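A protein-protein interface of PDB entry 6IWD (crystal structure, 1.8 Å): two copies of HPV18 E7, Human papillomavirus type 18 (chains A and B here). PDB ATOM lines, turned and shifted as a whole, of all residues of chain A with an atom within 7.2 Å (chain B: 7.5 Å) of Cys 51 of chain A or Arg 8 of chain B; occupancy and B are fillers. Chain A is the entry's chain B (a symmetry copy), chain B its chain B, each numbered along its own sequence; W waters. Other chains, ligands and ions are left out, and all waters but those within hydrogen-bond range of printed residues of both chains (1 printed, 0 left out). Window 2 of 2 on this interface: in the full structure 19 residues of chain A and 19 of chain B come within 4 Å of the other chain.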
ATOM      1  N   CYS A  15      26.921  17.889 -14.825  1.00  0.00           N
ATOM      2  CA  CYS A  15      25.699  17.098 -14.850  1.00  0.00           C
ATOM      3  C   CYS A  15      25.952  15.733 -14.221  1.00  0.00           C
ATOM      4  O   CYS A  15      26.970  15.087 -14.483  1.00  0.00           O
ATOM      5  CB  CYS A  15      25.191  16.928 -16.279  1.00  0.00           C
ATOM      6  SG  CYS A  15      23.762  15.819 -16.384  1.00  0.00           S
ATOM      7  N   CYS A  16      25.021  15.296 -13.377  1.00  0.00           N
ATOM      8  CA  CYS A  16      25.200  14.015 -12.709  1.00  0.00           C
ATOM      9  C   CYS A  16      24.884  12.830 -13.609  1.00  0.00           C
ATOM     10  O   CYS A  16      24.985  11.687 -13.152  1.00  0.00           O
ATOM     11  CB  CYS A  16      24.349  13.950 -11.440  1.00  0.00           C
ATOM     12  SG  CYS A  16      22.572  14.145 -11.686  1.00  0.00           S
ATOM     13  N   LYS A  17      24.522  13.067 -14.869  1.00  0.00           N
ATOM     14  CA  LYS A  17      24.211  11.983 -15.791  1.00  0.00           C
ATOM     15  C   LYS A  17      25.177  11.859 -16.958  1.00  0.00           C
ATOM     16  O   LYS A  17      25.326  10.758 -17.491  1.00  0.00           O
ATOM     17  CB  LYS A  17      22.792  12.147 -16.354  1.00  0.00           C
ATOM     18  CG  LYS A  17      21.697  12.073 -15.307  1.00  0.00           C
ATOM     19  CD  LYS A  17      21.773  10.765 -14.531  1.00  0.00           C
ATOM     20  CE  LYS A  17      21.477  10.996 -13.061  1.00  0.00           C
ATOM     21  NZ  LYS A  17      22.354  10.182 -12.159  1.00  0.00           N
ATOM     22  N   CYS A  18      25.849  12.940 -17.367  1.00  0.00           N
ATOM     23  CA  CYS A  18      26.543  12.911 -18.649  1.00  0.00           C
ATOM     24  C   CYS A  18      27.859  13.678 -18.701  1.00  0.00           C
ATOM     25  O   CYS A  18      28.397  13.857 -19.802  1.00  0.00           O
ATOM     26  CB  CYS A  18      25.637  13.461 -19.746  1.00  0.00           C
ATOM     27  SG  CYS A  18      25.679  15.259 -19.839  1.00  0.00           S
ATOM     28  N   GLU A  19      28.387  14.161 -17.578  1.00  0.00           N
ATOM     29  CA  GLU A  19      29.700  14.801 -17.508  1.00  0.00           C
ATOM     30  C   GLU A  19      29.740  16.187 -18.156  1.00  0.00           C
ATOM     31  O   GLU A  19      30.784  16.853 -18.089  1.00  0.00           O
ATOM     32  CB  GLU A  19      30.796  13.927 -18.141  1.00  0.00           C
ATOM     33  CG  GLU A  19      32.105  13.816 -17.375  1.00  0.00           C
ATOM     34  CD  GLU A  19      32.957  12.652 -17.873  1.00  0.00           C
ATOM     35  OE1 GLU A  19      34.160  12.850 -18.153  1.00  0.00           O
ATOM     36  OE2 GLU A  19      32.416  11.534 -17.992  1.00  0.00           O
ATOM     37  N   ALA A  20      28.661  16.648 -18.783  1.00  0.00           N
ATOM     38  CA  ALA A  20      28.667  17.992 -19.346  1.00  0.00           C
ATOM     39  C   ALA A  20      28.708  19.033 -18.234  1.00  0.00           C
ATOM     40  O   ALA A  20      28.167  18.828 -17.144  1.00  0.00           O
ATOM     41  CB  ALA A  20      27.440  18.226 -20.225  1.00  0.00           C
ATOM     42  N   VAL A  47      20.980  18.195 -13.266  1.00  0.00           N
ATOM     43  CA  VAL A  47      20.845  17.444 -14.507  1.00  0.00           C
ATOM     44  C   VAL A  47      20.789  18.447 -15.653  1.00  0.00           C
ATOM     45  O   VAL A  47      19.992  19.392 -15.612  1.00  0.00           O
ATOM     46  CB  VAL A  47      19.586  16.559 -14.491  1.00  0.00           C
ATOM     47  CG1 VAL A  47      19.513  15.723 -15.749  1.00  0.00           C
ATOM     48  CG2 VAL A  47      19.563  15.673 -13.244  1.00  0.00           C
ATOM     49  N   CYS A  48      21.633  18.246 -16.666  1.00  0.00           N
ATOM     50  CA  CYS A  48      21.671  19.173 -17.787  1.00  0.00           C
ATOM     51  C   CYS A  48      20.357  19.100 -18.562  1.00  0.00           C
ATOM     52  O   CYS A  48      19.571  18.169 -18.376  1.00  0.00           O
ATOM     53  CB  CYS A  48      22.877  18.884 -18.691  1.00  0.00           C
ATOM     54  SG  CYS A  48      22.812  17.395 -19.732  1.00  0.00           S
ATOM     55  N   PRO A  49      20.063  20.104 -19.396  1.00  0.00           N
ATOM     56  CA  PRO A  49      18.769  20.087 -20.100  1.00  0.00           C
ATOM     57  C   PRO A  49      18.587  18.875 -20.990  1.00  0.00           C
ATOM     58  O   PRO A  49      17.484  18.318 -21.051  1.00  0.00           O
ATOM     59  CB  PRO A  49      18.795  21.391 -20.904  1.00  0.00           C
ATOM     60  CG  PRO A  49      19.676  22.289 -20.104  1.00  0.00           C
ATOM     61  CD  PRO A  49      20.759  21.390 -19.572  1.00  0.00           C
ATOM     62  N   TRP A  50      19.648  18.432 -21.669  1.00  0.00           N
ATOM     63  CA  TRP A  50      19.510  17.285 -22.561  1.00  0.00           C
ATOM     64  C   TRP A  50      19.124  16.029 -21.790  1.00  0.00           C
ATOM     65  O   TRP A  50      18.146  15.353 -22.132  1.00  0.00           O
ATOM     66  CB  TRP A  50      20.798  17.053 -23.352  1.00  0.00           C
ATOM     67  CG  TRP A  50      20.576  16.025 -24.417  1.00  0.00           C
ATOM     68  CD1 TRP A  50      20.226  16.261 -25.715  1.00  0.00           C
ATOM     69  CD2 TRP A  50      20.626  14.600 -24.268  1.00  0.00           C
ATOM     70  NE1 TRP A  50      20.073  15.076 -26.385  1.00  0.00           N
ATOM     71  CE2 TRP A  50      20.311  14.041 -25.520  1.00  0.00           C
ATOM     72  CE3 TRP A  50      20.916  13.744 -23.201  1.00  0.00           C
ATOM     73  CZ2 TRP A  50      20.278  12.674 -25.739  1.00  0.00           C
ATOM     74  CZ3 TRP A  50      20.879  12.390 -23.417  1.00  0.00           C
ATOM     75  CH2 TRP A  50      20.564  11.864 -24.677  1.00  0.00           C
ATOM     76  N   CYS A  51      19.880  15.699 -20.737  1.00  0.00           N
ATOM     77  CA  CYS A  51      19.551  14.536 -19.919  1.00  0.00           C
ATOM     78  C   CYS A  51      18.186  14.659 -19.259  1.00  0.00           C
ATOM     79  O   CYS A  51      17.588  13.639 -18.898  1.00  0.00           O
ATOM     80  CB  CYS A  51      20.617  14.324 -18.851  1.00  0.00           C
ATOM     81  SG  CYS A  51      22.192  13.824 -19.524  1.00  0.00           S
ATOM     82  N   ALA A  52      17.691  15.885 -19.087  1.00  0.00           N
ATOM     83  CA  ALA A  52      16.372  16.081 -18.501  1.00  0.00           C
ATOM     84  C   ALA A  52      15.261  15.677 -19.465  1.00  0.00           C
ATOM     85  O   ALA A  52      14.175  15.282 -19.025  1.00  0.00           O
ATOM     86  CB  ALA A  52      16.208  17.539 -18.071  1.00  0.00           C
ATOM     87  N   SER A  53      15.515  15.756 -20.770  1.00  0.00           N
ATOM     88  CA  SER A  53      14.515  15.394 -21.775  1.00  0.00           C
ATOM     89  C   SER A  53      14.768  13.995 -22.325  1.00  0.00           C
ATOM     90  O   SER A  53      14.696  13.010 -21.588  1.00  0.00           O
ATOM     91  CB  SER A  53      14.500  16.423 -22.912  1.00  0.00           C
ATOM     92  OG  SER A  53      15.791  16.607 -23.468  1.00  0.00           O
ATOM     93  N   GLU B   5      18.135   6.767  -1.200  1.00  0.00           N
ATOM     94  CA  GLU B   5      18.907   7.188  -2.365  1.00  0.00           C
ATOM     95  C   GLU B   5      18.337   8.488  -2.944  1.00  0.00           C
ATOM     96  O   GLU B   5      17.130   8.723  -2.852  1.00  0.00           O
ATOM     97  CB  GLU B   5      18.927   6.071  -3.423  1.00  0.00           C
ATOM     98  CG  GLU B   5      19.827   6.351  -4.629  1.00  0.00           C
ATOM     99  CD  GLU B   5      20.337   5.093  -5.309  1.00  0.00           C
ATOM    100  OE1 GLU B   5      20.898   4.219  -4.611  1.00  0.00           O
ATOM    101  OE2 GLU B   5      20.193   4.989  -6.547  1.00  0.00           O
ATOM    102  N   PRO B   6      19.206   9.341  -3.494  1.00  0.00           N
ATOM    103  CA  PRO B   6      18.731  10.564  -4.157  1.00  0.00           C
ATOM    104  C   PRO B   6      17.644  10.285  -5.189  1.00  0.00           C
ATOM    105  O   PRO B   6      17.646   9.255  -5.870  1.00  0.00           O
ATOM    106  CB  PRO B   6      20.000  11.116  -4.814  1.00  0.00           C
ATOM    107  CG  PRO B   6      21.092  10.684  -3.909  1.00  0.00           C
ATOM    108  CD  PRO B   6      20.675   9.335  -3.350  1.00  0.00           C
ATOM    109  N   GLN B   7      16.703  11.219  -5.295  1.00  0.00           N
ATOM    110  CA  GLN B   7      15.634  11.152  -6.278  1.00  0.00           C
ATOM    111  C   GLN B   7      15.690  12.376  -7.181  1.00  0.00           C
ATOM    112  O   GLN B   7      16.324  13.386  -6.859  1.00  0.00           O
ATOM    113  CB  GLN B   7      14.259  11.052  -5.601  1.00  0.00           C
ATOM    114  CG  GLN B   7      14.003   9.716  -4.901  1.00  0.00           C
ATOM    115  CD  GLN B   7      13.810   8.557  -5.877  1.00  0.00           C
ATOM    116  OE1 GLN B   7      14.687   8.249  -6.685  1.00  0.00           O
ATOM    117  NE2 GLN B   7      12.654   7.906  -5.796  1.00  0.00           N
ATOM    118  N   ARG B   8      15.031  12.273  -8.328  1.00  0.00           N
ATOM    119  CA  ARG B   8      14.963  13.386  -9.262  1.00  0.00           C
ATOM    120  C   ARG B   8      13.800  14.296  -8.886  1.00  0.00           C
ATOM    121  O   ARG B   8      12.691  13.816  -8.624  1.00  0.00           O
ATOM    122  CB  ARG B   8      14.806  12.890 -10.698  1.00  0.00           C
ATOM    123  CG  ARG B   8      14.372  13.981 -11.656  1.00  0.00           C
ATOM    124  CD  ARG B   8      14.986  13.824 -13.021  1.00  0.00           C
ATOM    125  NE  ARG B   8      16.112  12.893 -13.023  1.00  0.00           N
ATOM    126  CZ  ARG B   8      16.809  12.597 -14.114  1.00  0.00           C
ATOM    127  NH1 ARG B   8      16.490  13.171 -15.268  1.00  0.00           N
ATOM    128  NH2 ARG B   8      17.822  11.738 -14.056  1.00  0.00           N
ATOM    129  N   HIS B   9      14.064  15.604  -8.847  1.00  0.00           N
ATOM    130  CA  HIS B   9      13.054  16.608  -8.548  1.00  0.00           C
ATOM    131  C   HIS B   9      13.181  17.754  -9.537  1.00  0.00           C
ATOM    132  O   HIS B   9      14.275  18.049 -10.025  1.00  0.00           O
ATOM    133  CB  HIS B   9      13.192  17.150  -7.122  1.00  0.00           C
ATOM    134  CG  HIS B   9      13.405  16.090  -6.092  1.00  0.00           C
ATOM    135  ND1 HIS B   9      12.365  15.368  -5.544  1.00  0.00           N
ATOM    136  CD2 HIS B   9      14.535  15.629  -5.504  1.00  0.00           C
ATOM    137  CE1 HIS B   9      12.848  14.502  -4.670  1.00  0.00           C
ATOM    138  NE2 HIS B   9      14.161  14.639  -4.626  1.00  0.00           N
ATOM    139  N   THR B  10      12.061  18.406  -9.833  1.00  0.00           N
ATOM    140  CA  THR B  10      12.073  19.585 -10.686  1.00  0.00           C
ATOM    141  C   THR B  10      11.677  20.806  -9.868  1.00  0.00           C
ATOM    142  O   THR B  10      10.680  20.775  -9.142  1.00  0.00           O
ATOM    143  CB  THR B  10      11.138  19.430 -11.889  1.00  0.00           C
ATOM    144  OG1 THR B  10      11.545  18.297 -12.659  1.00  0.00           O
ATOM    145  CG2 THR B  10      11.210  20.673 -12.781  1.00  0.00           C
ATOM    146  N   VAL B  25      16.373  20.931 -12.815  1.00  0.00           N
ATOM    147  CA  VAL B  25      16.205  19.511 -12.546  1.00  0.00           C
ATOM    148  C   VAL B  25      17.394  19.058 -11.715  1.00  0.00           C
ATOM    149  O   VAL B  25      18.548  19.190 -12.147  1.00  0.00           O
ATOM    150  CB  VAL B  25      16.078  18.703 -13.846  1.00  0.00           C
ATOM    151  CG1 VAL B  25      15.921  17.222 -13.540  1.00  0.00           C
ATOM    152  CG2 VAL B  25      14.897  19.228 -14.663  1.00  0.00           C
ATOM    153  N   VAL B  26      17.121  18.555 -10.518  1.00  0.00           N
ATOM    154  CA  VAL B  26      18.169  18.123  -9.608  1.00  0.00           C
ATOM    155  C   VAL B  26      17.939  16.668  -9.213  1.00  0.00           C
ATOM    156  O   VAL B  26      16.841  16.120  -9.340  1.00  0.00           O
ATOM    157  CB  VAL B  26      18.246  19.016  -8.348  1.00  0.00           C
ATOM    158  CG1 VAL B  26      18.664  20.431  -8.726  1.00  0.00           C
ATOM    159  CG2 VAL B  26      16.911  19.034  -7.617  1.00  0.00           C
ATOM    160  N   GLU B  27      19.003  16.045  -8.722  1.00  0.00           N
ATOM    161  CA  GLU B  27      18.911  14.800  -7.975  1.00  0.00           C
ATOM    162  C   GLU B  27      19.539  15.049  -6.617  1.00  0.00           C
ATOM    163  O   GLU B  27      20.624  15.639  -6.535  1.00  0.00           O
ATOM    164  CB  GLU B  27      19.607  13.647  -8.697  1.00  0.00           C
ATOM    165  CG  GLU B  27      18.978  13.333 -10.030  1.00  0.00           C
ATOM    166  CD  GLU B  27      19.404  11.985 -10.573  1.00  0.00           C
ATOM    167  OE1 GLU B  27      20.389  11.414 -10.052  1.00  0.00           O
ATOM    168  OE2 GLU B  27      18.747  11.495 -11.520  1.00  0.00           O
ATOM    169  N   SER B  28      18.848  14.642  -5.557  1.00  0.00           N
ATOM    170  CA  SER B  28      19.333  14.936  -4.212  1.00  0.00           C
ATOM    171  C   SER B  28      18.532  14.128  -3.203  1.00  0.00           C
ATOM    172  O   SER B  28      17.486  13.553  -3.522  1.00  0.00           O
ATOM    173  CB  SER B  28      19.224  16.431  -3.892  1.00  0.00           C
ATOM    174  OG  SER B  28      17.869  16.783  -3.689  1.00  0.00           O
ATOM    175  N   LEU B  33      16.970  18.657  -0.752  1.00  0.00           N
ATOM    176  CA  LEU B  33      15.908  19.309  -1.506  1.00  0.00           C
ATOM    177  C   LEU B  33      15.226  20.379  -0.660  1.00  0.00           C
ATOM    178  O   LEU B  33      15.000  21.500  -1.126  1.00  0.00           O
ATOM    179  CB  LEU B  33      14.892  18.272  -2.002  1.00  0.00           C
ATOM    180  CG  LEU B  33      13.639  18.914  -2.617  1.00  0.00           C
ATOM    181  CD1 LEU B  33      13.975  19.723  -3.851  1.00  0.00           C
ATOM    182  CD2 LEU B  33      12.576  17.869  -2.947  1.00  0.00           C
HETATM  183  O   HOH W   1      18.822  21.747 -14.319  1.00  0.00           O
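The guanidinium group of Arg 8 of chain B lies within salt-bridge range of the side-chain carboxylate of Glu 27 of chain B (2.7 Å).
N of Lys 17 of chain A sits close to SG of Cys 15 of chain A, 3.2 Å away.
Glu 27 of chain B touches Cys 16 of chain A.
NH2 of Arg 8 of chain B touches CE of Lys 17 of chain A (3.9 Å).
Val 47 of chain A touches Arg 8 of chain B.
Cys 51 of chain A touches Arg 8 of chain B.
Of the 13 printed residues of chain A, 4 touch a printed residue of chain B.
Hydrophobic or aromatic side chains of chain A within 4 Å of the printed part of chain B: Val 47.
Among the printed residues, Asp or Glu carboxylates within 4 Å of a Lys or Arg side-chain nitrogen of the other chain: Lys 17 of chain A with Glu 27 of chain B (3.1 Å).
OE1 of Glu 27 of chain B lies within salt-bridge range of NZ of Lys 17 of chain A (3.1 Å).
O of Val 25 of chain B is in hydrogen-bond range of N of Val 47 of chain A (2.9 Å).
No position is printed for both chains.
Of the 6 pairs that touch across the chains among the printed residues, none has its exchanged pair printed and touching as well.
Of the printed residues of chain B, Lys 17 of chain A touches Arg 8 and Glu 27.
Printed residues of chain B within 4 Å of Val 47 of chain A: Arg 8 (3.99 Å) and Val 25 (2.9 Å).
Of chain B, only Arg 8 comes within 4 Å of Cys 51 of chain A.
Of the printed residues of chain A, Arg 8 of chain B touches Lys 17, Val 47 and Cys 51.
Val 26 of chain B touches none of the printed residues of chain A.
Printed residues of chain A within 4 Å of Glu 27 of chain B: Cys 16 (3.9 Å) and Lys 17 (3.1 Å).
The nearest printed residue of chain B that does not touch Val 47 of chain A is Glu 27 of chain B (4.02 Å).
Water W1 bridges the backbone carbonyl oxygen of Val 47 of chain A (2.9 Å) and the backbone NH of Val 25 of chain B (3.0 Å).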
